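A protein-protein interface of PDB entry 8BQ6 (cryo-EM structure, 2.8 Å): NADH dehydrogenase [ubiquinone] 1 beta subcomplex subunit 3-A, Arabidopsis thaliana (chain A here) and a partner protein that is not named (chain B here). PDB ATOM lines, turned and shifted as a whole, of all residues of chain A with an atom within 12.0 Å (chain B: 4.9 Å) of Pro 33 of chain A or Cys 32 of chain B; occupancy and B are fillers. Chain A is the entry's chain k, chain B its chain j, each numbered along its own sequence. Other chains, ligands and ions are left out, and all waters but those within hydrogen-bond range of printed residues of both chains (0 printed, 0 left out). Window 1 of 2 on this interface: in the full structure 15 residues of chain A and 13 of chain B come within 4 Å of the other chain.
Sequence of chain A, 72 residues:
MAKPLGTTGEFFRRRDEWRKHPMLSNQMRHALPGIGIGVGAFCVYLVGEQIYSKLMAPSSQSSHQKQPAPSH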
ATOM      1  N   ASN A  26       2.022  20.159  20.456  1.00  0.00           N
ATOM      2  CA  ASN A  26       1.308  20.079  21.729  1.00  0.00           C
ATOM      3  C   ASN A  26      -0.059  19.424  21.558  1.00  0.00           C
ATOM      4  O   ASN A  26      -1.067  19.897  22.085  1.00  0.00           O
ATOM      5  CB  ASN A  26       1.172  21.460  22.372  1.00  0.00           C
ATOM      6  CG  ASN A  26       2.044  21.619  23.596  1.00  0.00           C
ATOM      7  OD1 ASN A  26       3.078  20.965  23.722  1.00  0.00           O
ATOM      8  ND2 ASN A  26       1.631  22.491  24.508  1.00  0.00           N
ATOM      9  N   GLN A  27      -0.097  18.318  20.821  1.00  0.00           N
ATOM     10  CA  GLN A  27      -1.369  17.686  20.505  1.00  0.00           C
ATOM     11  C   GLN A  27      -1.895  16.800  21.626  1.00  0.00           C
ATOM     12  O   GLN A  27      -3.007  16.277  21.505  1.00  0.00           O
ATOM     13  CB  GLN A  27      -1.244  16.868  19.222  1.00  0.00           C
ATOM     14  CG  GLN A  27      -1.033  17.700  17.972  1.00  0.00           C
ATOM     15  CD  GLN A  27      -2.141  18.703  17.740  1.00  0.00           C
ATOM     16  OE1 GLN A  27      -3.320  18.395  17.916  1.00  0.00           O
ATOM     17  NE2 GLN A  27      -1.770  19.903  17.315  1.00  0.00           N
ATOM     18  N   MET A  28      -1.133  16.612  22.704  1.00  0.00           N
ATOM     19  CA  MET A  28      -1.611  15.775  23.796  1.00  0.00           C
ATOM     20  C   MET A  28      -2.667  16.478  24.638  1.00  0.00           C
ATOM     21  O   MET A  28      -3.412  15.809  25.361  1.00  0.00           O
ATOM     22  CB  MET A  28      -0.434  15.329  24.672  1.00  0.00           C
ATOM     23  CG  MET A  28      -0.747  14.181  25.638  1.00  0.00           C
ATOM     24  SD  MET A  28      -0.878  12.515  24.935  1.00  0.00           S
ATOM     25  CE  MET A  28      -0.140  12.708  23.316  1.00  0.00           C
ATOM     26  N   ARG A  29      -2.754  17.806  24.557  1.00  0.00           N
ATOM     27  CA  ARG A  29      -3.820  18.527  25.236  1.00  0.00           C
ATOM     28  C   ARG A  29      -5.144  18.432  24.495  1.00  0.00           C
ATOM     29  O   ARG A  29      -6.160  18.918  25.005  1.00  0.00           O
ATOM     30  CB  ARG A  29      -3.422  19.988  25.422  1.00  0.00           C
ATOM     31  CG  ARG A  29      -1.926  20.184  25.520  1.00  0.00           C
ATOM     32  CD  ARG A  29      -1.525  21.536  24.988  1.00  0.00           C
ATOM     33  NE  ARG A  29      -2.222  21.859  23.750  1.00  0.00           N
ATOM     34  CZ  ARG A  29      -2.187  23.047  23.164  1.00  0.00           C
ATOM     35  NH1 ARG A  29      -1.465  24.038  23.658  1.00  0.00           N
ATOM     36  NH2 ARG A  29      -2.898  23.246  22.058  1.00  0.00           N
ATOM     37  N   HIS A  30      -5.153  17.839  23.304  1.00  0.00           N
ATOM     38  CA  HIS A  30      -6.375  17.534  22.579  1.00  0.00           C
ATOM     39  C   HIS A  30      -6.722  16.053  22.640  1.00  0.00           C
ATOM     40  O   HIS A  30      -7.679  15.622  21.990  1.00  0.00           O
ATOM     41  CB  HIS A  30      -6.246  17.989  21.124  1.00  0.00           C
ATOM     42  CG  HIS A  30      -6.345  19.472  20.947  1.00  0.00           C
ATOM     43  ND1 HIS A  30      -5.276  20.319  21.146  1.00  0.00           N
ATOM     44  CD2 HIS A  30      -7.387  20.259  20.587  1.00  0.00           C
ATOM     45  CE1 HIS A  30      -5.655  21.564  20.919  1.00  0.00           C
ATOM     46  NE2 HIS A  30      -6.930  21.555  20.576  1.00  0.00           N
ATOM     47  N   ALA A  31      -5.978  15.274  23.430  1.00  0.00           N
ATOM     48  CA  ALA A  31      -6.134  13.823  23.432  1.00  0.00           C
ATOM     49  C   ALA A  31      -7.526  13.389  23.867  1.00  0.00           C
ATOM     50  O   ALA A  31      -8.063  12.412  23.333  1.00  0.00           O
ATOM     51  CB  ALA A  31      -5.083  13.184  24.338  1.00  0.00           C
ATOM     52  N   LEU A  32      -8.135  14.094  24.818  1.00  0.00           N
ATOM     53  CA  LEU A  32      -9.414  13.691  25.396  1.00  0.00           C
ATOM     54  C   LEU A  32     -10.421  14.818  25.216  1.00  0.00           C
ATOM     55  O   LEU A  32     -10.756  15.528  26.173  1.00  0.00           O
ATOM     56  CB  LEU A  32      -9.264  13.329  26.871  1.00  0.00           C
ATOM     57  CG  LEU A  32      -8.291  12.193  27.169  1.00  0.00           C
ATOM     58  CD1 LEU A  32      -6.965  12.758  27.638  1.00  0.00           C
ATOM     59  CD2 LEU A  32      -8.870  11.258  28.211  1.00  0.00           C
ATOM     60  N   PRO A  33     -10.935  15.002  24.003  1.00  0.00           N
ATOM     61  CA  PRO A  33     -11.925  16.056  23.787  1.00  0.00           C
ATOM     62  C   PRO A  33     -13.220  15.716  24.502  1.00  0.00           C
ATOM     63  O   PRO A  33     -13.527  14.547  24.744  1.00  0.00           O
ATOM     64  CB  PRO A  33     -12.103  16.075  22.265  1.00  0.00           C
ATOM     65  CG  PRO A  33     -11.753  14.696  21.827  1.00  0.00           C
ATOM     66  CD  PRO A  33     -10.847  14.077  22.859  1.00  0.00           C
ATOM     67  N   GLY A  34     -13.967  16.753  24.867  1.00  0.00           N
ATOM     68  CA  GLY A  34     -15.204  16.542  25.583  1.00  0.00           C
ATOM     69  C   GLY A  34     -15.047  15.990  26.979  1.00  0.00           C
ATOM     70  O   GLY A  34     -16.035  15.537  27.563  1.00  0.00           O
ATOM     71  N   ILE A  35     -13.831  15.996  27.531  1.00  0.00           N
ATOM     72  CA  ILE A  35     -13.636  15.493  28.886  1.00  0.00           C
ATOM     73  C   ILE A  35     -14.230  16.446  29.918  1.00  0.00           C
ATOM     74  O   ILE A  35     -14.899  16.007  30.861  1.00  0.00           O
ATOM     75  CB  ILE A  35     -12.139  15.217  29.143  1.00  0.00           C
ATOM     76  CG1 ILE A  35     -11.956  14.456  30.457  1.00  0.00           C
ATOM     77  CG2 ILE A  35     -11.311  16.501  29.109  1.00  0.00           C
ATOM     78  CD1 ILE A  35     -12.640  13.111  30.473  1.00  0.00           C
ATOM     79  N   GLY A  36     -14.005  17.750  29.767  1.00  0.00           N
ATOM     80  CA  GLY A  36     -14.513  18.719  30.714  1.00  0.00           C
ATOM     81  C   GLY A  36     -16.021  18.830  30.674  1.00  0.00           C
ATOM     82  O   GLY A  36     -16.675  18.922  31.717  1.00  0.00           O
ATOM     83  N   ILE A  37     -16.583  18.815  29.464  1.00  0.00           N
ATOM     84  CA  ILE A  37     -18.027  18.963  29.308  1.00  0.00           C
ATOM     85  C   ILE A  37     -18.755  17.735  29.838  1.00  0.00           C
ATOM     86  O   ILE A  37     -19.831  17.845  30.439  1.00  0.00           O
ATOM     87  CB  ILE A  37     -18.377  19.237  27.835  1.00  0.00           C
ATOM     88  CG1 ILE A  37     -17.497  20.359  27.284  1.00  0.00           C
ATOM     89  CG2 ILE A  37     -19.848  19.575  27.692  1.00  0.00           C
ATOM     90  CD1 ILE A  37     -16.907  20.056  25.930  1.00  0.00           C
ATOM     91  N   GLY A  38     -18.198  16.546  29.604  1.00  0.00           N
ATOM     92  CA  GLY A  38     -18.823  15.342  30.127  1.00  0.00           C
ATOM     93  C   GLY A  38     -18.794  15.287  31.641  1.00  0.00           C
ATOM     94  O   GLY A  38     -19.768  14.879  32.279  1.00  0.00           O
ATOM     95  N   VAL A  39     -17.669  15.688  32.235  1.00  0.00           N
ATOM     96  CA  VAL A  39     -17.577  15.767  33.688  1.00  0.00           C
ATOM     97  C   VAL A  39     -18.513  16.841  34.226  1.00  0.00           C
ATOM     98  O   VAL A  39     -19.221  16.626  35.217  1.00  0.00           O
ATOM     99  CB  VAL A  39     -16.116  16.013  34.103  1.00  0.00           C
ATOM    100  CG1 VAL A  39     -16.036  16.508  35.535  1.00  0.00           C
ATOM    101  CG2 VAL A  39     -15.303  14.742  33.924  1.00  0.00           C
ATOM    102  N   GLY A  40     -18.542  18.008  33.578  1.00  0.00           N
ATOM    103  CA  GLY A  40     -19.445  19.059  34.013  1.00  0.00           C
ATOM    104  C   GLY A  40     -20.892  18.609  34.019  1.00  0.00           C
ATOM    105  O   GLY A  40     -21.616  18.824  34.993  1.00  0.00           O
ATOM    106  N   ALA A  41     -21.325  17.952  32.940  1.00  0.00           N
ATOM    107  CA  ALA A  41     -22.688  17.434  32.885  1.00  0.00           C
ATOM    108  C   ALA A  41     -22.918  16.376  33.956  1.00  0.00           C
ATOM    109  O   ALA A  41     -24.011  16.285  34.525  1.00  0.00           O
ATOM    110  CB  ALA A  41     -22.978  16.863  31.497  1.00  0.00           C
ATOM    111  N   PHE A  42     -21.903  15.554  34.233  1.00  0.00           N
ATOM    112  CA  PHE A  42     -22.025  14.578  35.310  1.00  0.00           C
ATOM    113  C   PHE A  42     -22.133  15.266  36.666  1.00  0.00           C
ATOM    114  O   PHE A  42     -22.841  14.785  37.559  1.00  0.00           O
ATOM    115  CB  PHE A  42     -20.842  13.611  35.296  1.00  0.00           C
ATOM    116  CG  PHE A  42     -21.083  12.357  36.086  1.00  0.00           C
ATOM    117  CD1 PHE A  42     -22.242  11.622  35.910  1.00  0.00           C
ATOM    118  CD2 PHE A  42     -20.170  11.937  37.037  1.00  0.00           C
ATOM    119  CE1 PHE A  42     -22.471  10.476  36.645  1.00  0.00           C
ATOM    120  CE2 PHE A  42     -20.395  10.792  37.774  1.00  0.00           C
ATOM    121  CZ  PHE A  42     -21.547  10.062  37.579  1.00  0.00           C
ATOM    122  N   THR B  27     -19.215  18.844  16.833  1.00  0.00           N
ATOM    123  CA  THR B  27     -19.692  17.466  16.903  1.00  0.00           C
ATOM    124  C   THR B  27     -18.670  16.560  17.579  1.00  0.00           C
ATOM    125  O   THR B  27     -19.029  15.731  18.424  1.00  0.00           O
ATOM    126  CB  THR B  27     -20.027  16.958  15.499  1.00  0.00           C
ATOM    127  OG1 THR B  27     -20.162  15.537  15.522  1.00  0.00           O
ATOM    128  CG2 THR B  27     -18.934  17.280  14.533  1.00  0.00           C
ATOM    129  N   GLY B  28     -17.393  16.721  17.219  1.00  0.00           N
ATOM    130  CA  GLY B  28     -16.325  15.902  17.814  1.00  0.00           C
ATOM    131  C   GLY B  28     -16.310  16.027  19.322  1.00  0.00           C
ATOM    132  O   GLY B  28     -16.390  14.982  19.996  1.00  0.00           O
ATOM    133  N   LYS B  29     -16.230  17.265  19.829  1.00  0.00           N
ATOM    134  CA  LYS B  29     -16.228  17.479  21.273  1.00  0.00           C
ATOM    135  C   LYS B  29     -17.513  16.960  21.903  1.00  0.00           C
ATOM    136  O   LYS B  29     -17.496  16.363  22.984  1.00  0.00           O
ATOM    137  CB  LYS B  29     -16.060  18.967  21.588  1.00  0.00           C
ATOM    138  CG  LYS B  29     -14.773  19.590  21.094  1.00  0.00           C
ATOM    139  CD  LYS B  29     -14.967  21.084  20.902  1.00  0.00           C
ATOM    140  CE  LYS B  29     -14.850  21.842  22.216  1.00  0.00           C
ATOM    141  NZ  LYS B  29     -13.982  21.130  23.189  1.00  0.00           N
ATOM    142  N   GLY B  30     -18.645  17.206  21.242  1.00  0.00           N
ATOM    143  CA  GLY B  30     -19.923  16.822  21.813  1.00  0.00           C
ATOM    144  C   GLY B  30     -20.102  15.321  21.914  1.00  0.00           C
ATOM    145  O   GLY B  30     -20.565  14.812  22.939  1.00  0.00           O
ATOM    146  N   LEU B  31     -19.721  14.606  20.856  1.00  0.00           N
ATOM    147  CA  LEU B  31     -19.934  13.135  20.827  1.00  0.00           C
ATOM    148  C   LEU B  31     -19.066  12.470  21.897  1.00  0.00           C
ATOM    149  O   LEU B  31     -19.586  11.595  22.606  1.00  0.00           O
ATOM    150  CB  LEU B  31     -19.593  12.598  19.433  1.00  0.00           C
ATOM    151  CG  LEU B  31     -19.941  11.132  19.184  1.00  0.00           C
ATOM    152  CD1 LEU B  31     -20.342  10.899  17.736  1.00  0.00           C
ATOM    153  CD2 LEU B  31     -18.784  10.226  19.571  1.00  0.00           C
ATOM    154  N   CYS B  32     -17.800  12.868  22.000  1.00  0.00           N
ATOM    155  CA  CYS B  32     -16.931  12.303  23.064  1.00  0.00           C
ATOM    156  C   CYS B  32     -17.439  12.732  24.447  1.00  0.00           C
ATOM    157  O   CYS B  32     -17.411  11.894  25.327  1.00  0.00           O
ATOM    158  CB  CYS B  32     -15.477  12.706  22.864  1.00  0.00           C
ATOM    159  SG  CYS B  32     -14.541  11.530  21.854  1.00  0.00           S
ATOM    160  N   ALA B  33     -17.905  13.972  24.631  1.00  0.00           N
ATOM    161  CA  ALA B  33     -18.473  14.367  25.918  1.00  0.00           C
ATOM    162  C   ALA B  33     -19.679  13.509  26.267  1.00  0.00           C
ATOM    163  O   ALA B  33     -19.836  13.083  27.418  1.00  0.00           O
ATOM    164  CB  ALA B  33     -18.857  15.846  25.900  1.00  0.00           C
ATOM    165  N   VAL B  34     -20.535  13.238  25.280  1.00  0.00           N
ATOM    166  CA  VAL B  34     -21.644  12.307  25.471  1.00  0.00           C
ATOM    167  C   VAL B  34     -21.113  10.943  25.893  1.00  0.00           C
ATOM    168  O   VAL B  34     -21.720  10.242  26.712  1.00  0.00           O
ATOM    169  CB  VAL B  34     -22.474  12.225  24.174  1.00  0.00           C
ATOM    170  CG1 VAL B  34     -23.288  10.938  24.109  1.00  0.00           C
ATOM    171  CG2 VAL B  34     -23.355  13.455  24.020  1.00  0.00           C
ATOM    172  N   MET B  35     -19.954  10.561  25.350  1.00  0.00           N
ATOM    173  CA  MET B  35     -19.337   9.280  25.675  1.00  0.00           C
ATOM    174  C   MET B  35     -18.779   9.267  27.093  1.00  0.00           C
ATOM    175  O   MET B  35     -18.954   8.291  27.832  1.00  0.00           O
ATOM    176  CB  MET B  35     -18.231   8.984  24.664  1.00  0.00           C
ATOM    177  CG  MET B  35     -17.357   7.816  25.027  1.00  0.00           C
ATOM    178  SD  MET B  35     -15.766   7.888  24.200  1.00  0.00           S
ATOM    179  CE  MET B  35     -15.361   6.153  24.208  1.00  0.00           C
ATOM    180  N   TRP B  36     -18.073  10.333  27.481  1.00  0.00           N
ATOM    181  CA  TRP B  36     -17.513  10.397  28.828  1.00  0.00           C
ATOM    182  C   TRP B  36     -18.610  10.378  29.881  1.00  0.00           C
ATOM    183  O   TRP B  36     -18.493   9.687  30.899  1.00  0.00           O
ATOM    184  CB  TRP B  36     -16.654  11.649  28.982  1.00  0.00           C
ATOM    185  CG  TRP B  36     -15.493  11.672  28.061  1.00  0.00           C
ATOM    186  CD1 TRP B  36     -15.220  12.608  27.110  1.00  0.00           C
ATOM    187  CD2 TRP B  36     -14.434  10.715  28.000  1.00  0.00           C
ATOM    188  NE1 TRP B  36     -14.058  12.290  26.454  1.00  0.00           N
ATOM    189  CE2 TRP B  36     -13.553  11.132  26.984  1.00  0.00           C
ATOM    190  CE3 TRP B  36     -14.144   9.546  28.706  1.00  0.00           C
ATOM    191  CZ2 TRP B  36     -12.407  10.421  26.655  1.00  0.00           C
ATOM    192  CZ3 TRP B  36     -13.007   8.841  28.378  1.00  0.00           C
ATOM    193  CH2 TRP B  36     -12.151   9.281  27.364  1.00  0.00           C
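NE1 of Trp 36 of chain B is in hydrogen-bond range of O of Pro 33 of chain A, 2.9 Å away.
Leu 32 of chain A touches Trp 36 of chain B (CD2 to CH2, 3.9 Å). Pro 33 of chain A touches Cys 32 of chain B (O to CB, 3.3 Å). Gly 34 of chain A touches Lys 29 of chain B (CA to O, 3.5 Å). Gly 34 of chain A touches Ala 33 of chain B (O to CA, 3.2 Å). Gly 34 of chain A touches Trp 36 of chain B (O to CD1, 3.1 Å). Ile 35 of chain A touches Trp 36 of chain B. Ile 37 of chain A touches Ala 33 of chain B (CB to CB, 3.9 Å). Gly 38 of chain A touches Ala 33 of chain B.
Printed residues of chain B within 4 Å of Leu 32 of chain A: Trp 36. Pro 33 of chain A touches just these residues of chain B: Cys 32 and Trp 36. Of the printed residues of chain B, Gly 34 of chain A touches Lys 29 (3.5 Å), Ala 33 (3.2 Å) and Trp 36 (3.1 Å). No residue of chain A comes within 4 Å of Gly 28 of chain B. Of chain A, only Gly 34 (3.5 Å) comes within 4 Å of Lys 29 of chain B. No residue of chain A comes within 4 Å of Gly 30 of chain B. Of chain A, only Pro 33 comes within 4 Å of Cys 32 of chain B. Of chain A, only Gly 34, Ile 37 and Gly 38 come within 4 Å of Ala 33 of chain B. Val 34 of chain B touches none of the printed residues of chain A. No residue of chain A comes within 4 Å of Met 35 of chain B. Of chain A, only Leu 32 (3.9 Å), Pro 33 (2.9 Å), Gly 34 (3.1 Å) and Ile 35 (3.7 Å) come within 4 Å of Trp 36 of chain B. The nearest residue of chain A that does not touch Cys 32 of chain B is Gly 34 of chain A (4.4 Å). The nearest printed residue of chain B that does not touch Ile 35 of chain A is Ala 33 of chain B (5.2 Å).
Of the 17 printed residues of chain A, 6 touch a printed residue of chain B. Of the 10 printed residues of chain B, 4 touch a printed residue of chain A. Hydrophobic or aromatic side chains of chain B within 4 Å of the printed part of chain A: Ala 33 and Trp 36. Among the printed residues, 9 pairs touch across the chains. Among the printed residues, no Asp or Glu carboxylate lies within 4 Å of a Lys or Arg side-chain nitrogen of the other chain.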
